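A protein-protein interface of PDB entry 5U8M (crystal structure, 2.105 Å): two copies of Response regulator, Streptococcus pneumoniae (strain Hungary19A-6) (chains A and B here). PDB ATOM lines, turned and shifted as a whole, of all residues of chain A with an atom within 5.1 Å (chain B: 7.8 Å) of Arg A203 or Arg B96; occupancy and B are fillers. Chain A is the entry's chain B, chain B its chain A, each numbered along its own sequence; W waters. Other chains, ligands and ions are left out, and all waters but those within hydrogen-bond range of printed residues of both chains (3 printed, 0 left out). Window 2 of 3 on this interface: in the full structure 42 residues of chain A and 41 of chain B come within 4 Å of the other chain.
Water W1 bridges NH2 of Arg B96 (2.5 Å) and NH1 of Arg A203 (3.0 Å). Water W2 lies within hydrogen-bond range of O of Val B99 (2.7 Å), OH of Tyr A201 (3.0 Å) and O of Ala B98 (3.5 Å). Water W3 lies within hydrogen-bond range of OE2 of Glu A163 and O of Arg B96.
The backbone carbonyl oxygen (O) of Gln B95 sits at hydrogen-bond distance from the side-chain hydroxyl (OH) of Tyr A201, 2.7 Å away. OE2 of Glu B92 is in hydrogen-bond range of OH of Tyr A204, 2.8 Å away.
No position is printed for both chains. Of the 7 pairs that touch across the chains among the printed residues, none has its exchanged pair printed and touching as well.
Arg A203 touches just one residue of chain B: Arg B96 (3.8 Å). Of the printed residues of chain A, Arg B96 touches Thr A160 (3.2 Å), Arg A203 (3.8 Å) and Tyr A204 (3.1 Å). Printed residues of chain A within 4 Å of Glu B92: Tyr A204. Of the printed residues of chain A, Gln B95 touches Tyr A201 and Tyr A204. Glu B90 touches none of the printed residues of chain A. Ile A202 touches none of the printed residues of chain B. The nearest printed residue of chain B that does not touch Tyr A201 is Ala B98 (4.2 Å).
The side-chain carboxylate of Glu B92 is in salt-bridge range of the guanidinium group of Arg B96, at 3.6 Å. OG of Ser A207 sits at hydrogen-bond distance from O of Tyr A204, 3.0 Å away. The backbone NH (N) of Thr A160 sits at hydrogen-bond distance from the side-chain carboxylate (OE1) of Glu A163. The side-chain hydroxyl (OH) of Tyr B101 is in hydrogen-bond range of the side-chain amide nitrogen (NE2) of Gln B95, at 3.3 Å.
Thr A160 touches Pro B74. CG2 of Thr A160 touches O of Arg B96 (3.2 Å). Arg A203 touches Arg B96 (NH2 to NH2, 3.8 Å). Gln B95 touches Tyr A204. CD1 of Tyr A204 touches NH1 of Arg B96 (3.1 Å).
Of the 12 printed residues of chain A, 4 touch a printed residue of chain B. Hydrophobic or aromatic side chains of chain A that line the printed part of chain B: Tyr A201 and Tyr A204. Among the printed residues, 7 pairs touch across the chains.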
ATOM      1  N   THR A 160      11.595  17.374  -7.924  1.00  0.00           N
ATOM      2  CA  THR A 160      11.120  18.340  -8.890  1.00  0.00           C
ATOM      3  C   THR A 160      12.084  19.514  -8.913  1.00  0.00           C
ATOM      4  O   THR A 160      12.974  19.620  -8.082  1.00  0.00           O
ATOM      5  CB  THR A 160       9.739  18.834  -8.508  1.00  0.00           C
ATOM      6  OG1 THR A 160       9.862  19.574  -7.290  1.00  0.00           O
ATOM      7  CG2 THR A 160       8.794  17.660  -8.313  1.00  0.00           C
ATOM      8  N   GLU A 163      11.900  21.530  -5.642  1.00  0.00           N
ATOM      9  CA  GLU A 163      12.515  20.741  -4.586  1.00  0.00           C
ATOM     10  C   GLU A 163      14.041  20.726  -4.720  1.00  0.00           C
ATOM     11  O   GLU A 163      14.769  20.934  -3.741  1.00  0.00           O
ATOM     12  CB  GLU A 163      11.943  19.327  -4.649  1.00  0.00           C
ATOM     13  CG  GLU A 163      10.486  19.248  -4.270  1.00  0.00           C
ATOM     14  CD  GLU A 163       9.835  17.923  -4.637  1.00  0.00           C
ATOM     15  OE1 GLU A 163      10.471  17.099  -5.325  1.00  0.00           O
ATOM     16  OE2 GLU A 163       8.662  17.707  -4.260  1.00  0.00           O
ATOM     17  N   VAL A 198       6.936  27.715   1.661  1.00  0.00           N
ATOM     18  CA  VAL A 198       8.203  27.103   2.058  1.00  0.00           C
ATOM     19  C   VAL A 198       7.955  25.790   2.801  1.00  0.00           C
ATOM     20  O   VAL A 198       8.566  24.759   2.496  1.00  0.00           O
ATOM     21  CB  VAL A 198       9.023  28.077   2.920  1.00  0.00           C
ATOM     22  CG1 VAL A 198      10.270  27.393   3.455  1.00  0.00           C
ATOM     23  CG2 VAL A 198       9.405  29.327   2.152  1.00  0.00           C
ATOM     24  N   ASP A 199       7.041  25.806   3.786  1.00  0.00           N
ATOM     25  CA  ASP A 199       6.824  24.608   4.599  1.00  0.00           C
ATOM     26  C   ASP A 199       6.192  23.499   3.778  1.00  0.00           C
ATOM     27  O   ASP A 199       6.439  22.317   4.037  1.00  0.00           O
ATOM     28  CB  ASP A 199       5.957  24.927   5.827  1.00  0.00           C
ATOM     29  CG  ASP A 199       6.361  26.231   6.511  1.00  0.00           C
ATOM     30  OD1 ASP A 199       7.352  26.259   7.266  1.00  0.00           O
ATOM     31  OD2 ASP A 199       5.671  27.249   6.290  1.00  0.00           O
ATOM     32  N   VAL A 200       5.375  23.847   2.781  1.00  0.00           N
ATOM     33  CA  VAL A 200       4.857  22.826   1.881  1.00  0.00           C
ATOM     34  C   VAL A 200       6.005  22.084   1.199  1.00  0.00           C
ATOM     35  O   VAL A 200       5.987  20.852   1.086  1.00  0.00           O
ATOM     36  CB  VAL A 200       3.914  23.463   0.848  1.00  0.00           C
ATOM     37  CG1 VAL A 200       3.448  22.426  -0.159  1.00  0.00           C
ATOM     38  CG2 VAL A 200       2.744  24.143   1.563  1.00  0.00           C
ATOM     39  N   TYR A 201       7.000  22.826   0.701  1.00  0.00           N
ATOM     40  CA  TYR A 201       8.035  22.202  -0.129  1.00  0.00           C
ATOM     41  C   TYR A 201       9.119  21.536   0.720  1.00  0.00           C
ATOM     42  O   TYR A 201       9.621  20.482   0.321  1.00  0.00           O
ATOM     43  CB  TYR A 201       8.603  23.228  -1.137  1.00  0.00           C
ATOM     44  CG  TYR A 201       7.653  23.375  -2.305  1.00  0.00           C
ATOM     45  CD1 TYR A 201       6.598  24.261  -2.245  1.00  0.00           C
ATOM     46  CD2 TYR A 201       7.759  22.564  -3.435  1.00  0.00           C
ATOM     47  CE1 TYR A 201       5.692  24.375  -3.291  1.00  0.00           C
ATOM     48  CE2 TYR A 201       6.842  22.672  -4.494  1.00  0.00           C
ATOM     49  CZ  TYR A 201       5.809  23.581  -4.408  1.00  0.00           C
ATOM     50  OH  TYR A 201       4.857  23.711  -5.416  1.00  0.00           O
ATOM     51  N   ILE A 202       9.436  22.066   1.915  1.00  0.00           N
ATOM     52  CA  ILE A 202      10.213  21.277   2.878  1.00  0.00           C
ATOM     53  C   ILE A 202       9.597  19.889   3.030  1.00  0.00           C
ATOM     54  O   ILE A 202      10.284  18.858   2.965  1.00  0.00           O
ATOM     55  CB  ILE A 202      10.292  21.997   4.231  1.00  0.00           C
ATOM     56  CG1 ILE A 202      11.100  23.282   4.105  1.00  0.00           C
ATOM     57  CG2 ILE A 202      10.888  21.063   5.336  1.00  0.00           C
ATOM     58  CD1 ILE A 202      12.583  23.079   3.825  1.00  0.00           C
ATOM     59  N   ARG A 203       8.281  19.846   3.214  1.00  0.00           N
ATOM     60  CA  ARG A 203       7.607  18.574   3.430  1.00  0.00           C
ATOM     61  C   ARG A 203       7.681  17.697   2.195  1.00  0.00           C
ATOM     62  O   ARG A 203       7.863  16.479   2.301  1.00  0.00           O
ATOM     63  CB  ARG A 203       6.148  18.823   3.844  1.00  0.00           C
ATOM     64  CG  ARG A 203       5.416  17.593   4.375  1.00  0.00           C
ATOM     65  CD  ARG A 203       3.967  17.892   4.765  1.00  0.00           C
ATOM     66  NE  ARG A 203       3.101  18.118   3.606  1.00  0.00           N
ATOM     67  CZ  ARG A 203       2.600  17.152   2.839  1.00  0.00           C
ATOM     68  NH1 ARG A 203       2.874  15.881   3.093  1.00  0.00           N
ATOM     69  NH2 ARG A 203       1.827  17.457   1.810  1.00  0.00           N
ATOM     70  N   TYR A 204       7.500  18.290   1.010  1.00  0.00           N
ATOM     71  CA  TYR A 204       7.693  17.544  -0.211  1.00  0.00           C
ATOM     72  C   TYR A 204       9.108  16.986  -0.267  1.00  0.00           C
ATOM     73  O   TYR A 204       9.314  15.829  -0.650  1.00  0.00           O
ATOM     74  CB  TYR A 204       7.430  18.448  -1.416  1.00  0.00           C
ATOM     75  CG  TYR A 204       5.980  18.782  -1.705  1.00  0.00           C
ATOM     76  CD1 TYR A 204       4.947  18.035  -1.172  1.00  0.00           C
ATOM     77  CD2 TYR A 204       5.650  19.857  -2.539  1.00  0.00           C
ATOM     78  CE1 TYR A 204       3.630  18.348  -1.447  1.00  0.00           C
ATOM     79  CE2 TYR A 204       4.343  20.170  -2.817  1.00  0.00           C
ATOM     80  CZ  TYR A 204       3.338  19.414  -2.271  1.00  0.00           C
ATOM     81  OH  TYR A 204       2.033  19.724  -2.548  1.00  0.00           O
ATOM     82  N   LEU A 205      10.086  17.797   0.141  1.00  0.00           N
ATOM     83  CA  LEU A 205      11.485  17.412   0.040  1.00  0.00           C
ATOM     84  C   LEU A 205      11.783  16.260   0.988  1.00  0.00           C
ATOM     85  O   LEU A 205      12.276  15.208   0.557  1.00  0.00           O
ATOM     86  CB  LEU A 205      12.361  18.627   0.329  1.00  0.00           C
ATOM     87  CG  LEU A 205      13.869  18.524   0.197  1.00  0.00           C
ATOM     88  CD1 LEU A 205      14.314  18.030  -1.201  1.00  0.00           C
ATOM     89  CD2 LEU A 205      14.406  19.904   0.481  1.00  0.00           C
ATOM     90  N   ARG A 206      11.392  16.409   2.265  1.00  0.00           N
ATOM     91  CA  ARG A 206      11.589  15.345   3.248  1.00  0.00           C
ATOM     92  C   ARG A 206      10.982  14.041   2.778  1.00  0.00           C
ATOM     93  O   ARG A 206      11.591  12.976   2.921  1.00  0.00           O
ATOM     94  CB  ARG A 206      10.990  15.723   4.598  1.00  0.00           C
ATOM     95  CG  ARG A 206      11.805  16.727   5.417  1.00  0.00           C
ATOM     96  CD  ARG A 206      11.402  16.705   6.899  1.00  0.00           C
ATOM     97  NE  ARG A 206      12.324  17.464   7.750  1.00  0.00           N
ATOM     98  CZ  ARG A 206      12.030  18.577   8.434  1.00  0.00           C
ATOM     99  NH1 ARG A 206      10.826  19.113   8.386  1.00  0.00           N
ATOM    100  NH2 ARG A 206      12.957  19.165   9.183  1.00  0.00           N
ATOM    101  N   SER A 207       9.782  14.097   2.206  1.00  0.00           N
ATOM    102  CA  SER A 207       9.110  12.867   1.805  1.00  0.00           C
ATOM    103  C   SER A 207       9.804  12.180   0.636  1.00  0.00           C
ATOM    104  O   SER A 207       9.570  10.990   0.411  1.00  0.00           O
ATOM    105  CB  SER A 207       7.643  13.157   1.447  1.00  0.00           C
ATOM    106  OG  SER A 207       7.497  13.588   0.102  1.00  0.00           O
ATOM    107  N   ALA B  66       4.355  14.333 -16.630  1.00  0.00           N
ATOM    108  CA  ALA B  66       5.429  14.689 -15.710  1.00  0.00           C
ATOM    109  C   ALA B  66       6.063  13.448 -15.102  1.00  0.00           C
ATOM    110  O   ALA B  66       7.286  13.383 -14.945  1.00  0.00           O
ATOM    111  CB  ALA B  66       4.891  15.597 -14.605  1.00  0.00           C
ATOM    112  N   PRO B  74      14.142  14.608 -13.851  1.00  0.00           N
ATOM    113  CA  PRO B  74      13.231  14.783 -12.700  1.00  0.00           C
ATOM    114  C   PRO B  74      12.987  16.234 -12.329  1.00  0.00           C
ATOM    115  O   PRO B  74      11.950  16.541 -11.719  1.00  0.00           O
ATOM    116  CB  PRO B  74      13.946  14.033 -11.560  1.00  0.00           C
ATOM    117  CG  PRO B  74      15.401  13.994 -11.982  1.00  0.00           C
ATOM    118  CD  PRO B  74      15.380  13.902 -13.485  1.00  0.00           C
ATOM    119  N   GLU B  90      -7.449  19.211  -9.750  1.00  0.00           N
ATOM    120  CA  GLU B  90      -6.176  18.500  -9.714  1.00  0.00           C
ATOM    121  C   GLU B  90      -5.116  19.253  -8.921  1.00  0.00           C
ATOM    122  O   GLU B  90      -3.924  19.018  -9.130  1.00  0.00           O
ATOM    123  CB  GLU B  90      -5.653  18.256 -11.148  1.00  0.00           C
ATOM    124  CG  GLU B  90      -6.546  17.436 -12.080  1.00  0.00           C
ATOM    125  CD  GLU B  90      -6.801  16.011 -11.539  1.00  0.00           C
ATOM    126  OE1 GLU B  90      -5.938  15.496 -10.797  1.00  0.00           O
ATOM    127  OE2 GLU B  90      -7.870  15.427 -11.829  1.00  0.00           O
ATOM    128  N   LEU B  91      -5.504  20.153  -8.021  1.00  0.00           N
ATOM    129  CA  LEU B  91      -4.560  21.148  -7.521  1.00  0.00           C
ATOM    130  C   LEU B  91      -3.404  20.511  -6.749  1.00  0.00           C
ATOM    131  O   LEU B  91      -2.230  20.848  -6.973  1.00  0.00           O
ATOM    132  CB  LEU B  91      -5.275  22.165  -6.639  1.00  0.00           C
ATOM    133  CG  LEU B  91      -4.435  23.418  -6.348  1.00  0.00           C
ATOM    134  CD1 LEU B  91      -4.089  24.164  -7.613  1.00  0.00           C
ATOM    135  CD2 LEU B  91      -5.177  24.368  -5.419  1.00  0.00           C
ATOM    136  N   GLU B  92      -3.720  19.592  -5.836  1.00  0.00           N
ATOM    137  CA  GLU B  92      -2.694  19.009  -4.975  1.00  0.00           C
ATOM    138  C   GLU B  92      -1.612  18.333  -5.807  1.00  0.00           C
ATOM    139  O   GLU B  92      -0.417  18.552  -5.596  1.00  0.00           O
ATOM    140  CB  GLU B  92      -3.333  18.010  -4.011  1.00  0.00           C
ATOM    141  CG  GLU B  92      -2.330  17.268  -3.144  1.00  0.00           C
ATOM    142  CD  GLU B  92      -1.498  18.214  -2.295  1.00  0.00           C
ATOM    143  OE1 GLU B  92      -2.095  19.089  -1.629  1.00  0.00           O
ATOM    144  OE2 GLU B  92      -0.253  18.090  -2.303  1.00  0.00           O
ATOM    145  N   VAL B  93      -2.033  17.512  -6.766  1.00  0.00           N
ATOM    146  CA  VAL B  93      -1.135  16.869  -7.720  1.00  0.00           C
ATOM    147  C   VAL B  93      -0.333  17.911  -8.512  1.00  0.00           C
ATOM    148  O   VAL B  93       0.891  17.837  -8.618  1.00  0.00           O
ATOM    149  CB  VAL B  93      -1.975  15.973  -8.646  1.00  0.00           C
ATOM    150  CG1 VAL B  93      -1.155  15.372  -9.753  1.00  0.00           C
ATOM    151  CG2 VAL B  93      -2.697  14.880  -7.811  1.00  0.00           C
ATOM    152  N   VAL B  94      -1.007  18.891  -9.088  1.00  0.00           N
ATOM    153  CA  VAL B  94      -0.278  19.909  -9.843  1.00  0.00           C
ATOM    154  C   VAL B  94       0.767  20.599  -8.963  1.00  0.00           C
ATOM    155  O   VAL B  94       1.887  20.877  -9.406  1.00  0.00           O
ATOM    156  CB  VAL B  94      -1.266  20.919 -10.455  1.00  0.00           C
ATOM    157  CG1 VAL B  94      -0.527  22.130 -10.955  1.00  0.00           C
ATOM    158  CG2 VAL B  94      -2.035  20.271 -11.597  1.00  0.00           C
ATOM    159  N   GLN B  95       0.422  20.909  -7.714  1.00  0.00           N
ATOM    160  CA  GLN B  95       1.375  21.618  -6.860  1.00  0.00           C
ATOM    161  C   GLN B  95       2.650  20.808  -6.629  1.00  0.00           C
ATOM    162  O   GLN B  95       3.702  21.383  -6.311  1.00  0.00           O
ATOM    163  CB  GLN B  95       0.728  21.969  -5.530  1.00  0.00           C
ATOM    164  CG  GLN B  95       0.196  23.426  -5.429  1.00  0.00           C
ATOM    165  CD  GLN B  95      -0.985  23.580  -4.455  1.00  0.00           C
ATOM    166  OE1 GLN B  95      -1.390  22.623  -3.787  1.00  0.00           O
ATOM    167  NE2 GLN B  95      -1.551  24.795  -4.390  1.00  0.00           N
ATOM    168  N   ARG B  96       2.585  19.494  -6.817  1.00  0.00           N
ATOM    169  CA  ARG B  96       3.751  18.651  -6.592  1.00  0.00           C
ATOM    170  C   ARG B  96       4.645  18.617  -7.822  1.00  0.00           C
ATOM    171  O   ARG B  96       5.867  18.698  -7.686  1.00  0.00           O
ATOM    172  CB  ARG B  96       3.333  17.227  -6.218  1.00  0.00           C
ATOM    173  CG  ARG B  96       2.586  17.111  -4.898  1.00  0.00           C
ATOM    174  CD  ARG B  96       2.284  15.658  -4.543  1.00  0.00           C
ATOM    175  NE  ARG B  96       2.131  15.463  -3.100  1.00  0.00           N
ATOM    176  CZ  ARG B  96       3.144  15.311  -2.247  1.00  0.00           C
ATOM    177  NH1 ARG B  96       4.406  15.332  -2.670  1.00  0.00           N
ATOM    178  NH2 ARG B  96       2.893  15.142  -0.958  1.00  0.00           N
ATOM    179  N   PHE B  97       4.066  18.505  -9.031  1.00  0.00           N
ATOM    180  CA  PHE B  97       4.919  18.364 -10.212  1.00  0.00           C
ATOM    181  C   PHE B  97       5.204  19.662 -10.971  1.00  0.00           C
ATOM    182  O   PHE B  97       6.158  19.698 -11.765  1.00  0.00           O
ATOM    183  CB  PHE B  97       4.340  17.302 -11.155  1.00  0.00           C
ATOM    184  CG  PHE B  97       3.128  17.726 -11.955  1.00  0.00           C
ATOM    185  CD1 PHE B  97       3.275  18.488 -13.097  1.00  0.00           C
ATOM    186  CD2 PHE B  97       1.864  17.283 -11.613  1.00  0.00           C
ATOM    187  CE1 PHE B  97       2.181  18.836 -13.852  1.00  0.00           C
ATOM    188  CE2 PHE B  97       0.764  17.623 -12.357  1.00  0.00           C
ATOM    189  CZ  PHE B  97       0.926  18.411 -13.501  1.00  0.00           C
ATOM    190  N   ALA B  98       4.455  20.729 -10.735  1.00  0.00           N
ATOM    191  CA  ALA B  98       4.562  21.937 -11.545  1.00  0.00           C
ATOM    192  C   ALA B  98       5.365  22.992 -10.808  1.00  0.00           C
ATOM    193  O   ALA B  98       5.247  23.144  -9.590  1.00  0.00           O
ATOM    194  CB  ALA B  98       3.185  22.507 -11.904  1.00  0.00           C
ATOM    195  N   VAL B  99       6.208  23.706 -11.544  1.00  0.00           N
ATOM    196  CA  VAL B  99       6.960  24.798 -10.936  1.00  0.00           C
ATOM    197  C   VAL B  99       6.002  25.911 -10.534  1.00  0.00           C
ATOM    198  O   VAL B  99       6.230  26.631  -9.558  1.00  0.00           O
ATOM    199  CB  VAL B  99       8.053  25.249 -11.927  1.00  0.00           C
ATOM    200  CG1 VAL B  99       7.500  26.234 -12.989  1.00  0.00           C
ATOM    201  CG2 VAL B  99       9.186  25.856 -11.217  1.00  0.00           C
ATOM    202  N   TYR B 101       1.577  27.415 -11.386  1.00  0.00           N
ATOM    203  CA  TYR B 101       0.346  27.328 -12.152  1.00  0.00           C
ATOM    204  C   TYR B 101      -0.309  28.695 -12.228  1.00  0.00           C
ATOM    205  O   TYR B 101      -0.080  29.563 -11.390  1.00  0.00           O
ATOM    206  CB  TYR B 101      -0.608  26.310 -11.556  1.00  0.00           C
ATOM    207  CG  TYR B 101      -1.029  26.622 -10.143  1.00  0.00           C
ATOM    208  CD1 TYR B 101      -2.143  27.384  -9.903  1.00  0.00           C
ATOM    209  CD2 TYR B 101      -0.317  26.134  -9.050  1.00  0.00           C
ATOM    210  CE1 TYR B 101      -2.553  27.667  -8.604  1.00  0.00           C
ATOM    211  CE2 TYR B 101      -0.717  26.412  -7.743  1.00  0.00           C
ATOM    212  CZ  TYR B 101      -1.844  27.170  -7.540  1.00  0.00           C
ATOM    213  OH  TYR B 101      -2.254  27.470  -6.268  1.00  0.00           O
HETATM  214  O   HOH W   1       3.996  14.086   0.961  1.00  0.00           O
HETATM  215  O   HOH W   2       6.553  25.332  -7.247  1.00  0.00           O
HETATM  216  O   HOH W   3       6.604  16.162  -5.390  1.00  0.00           O
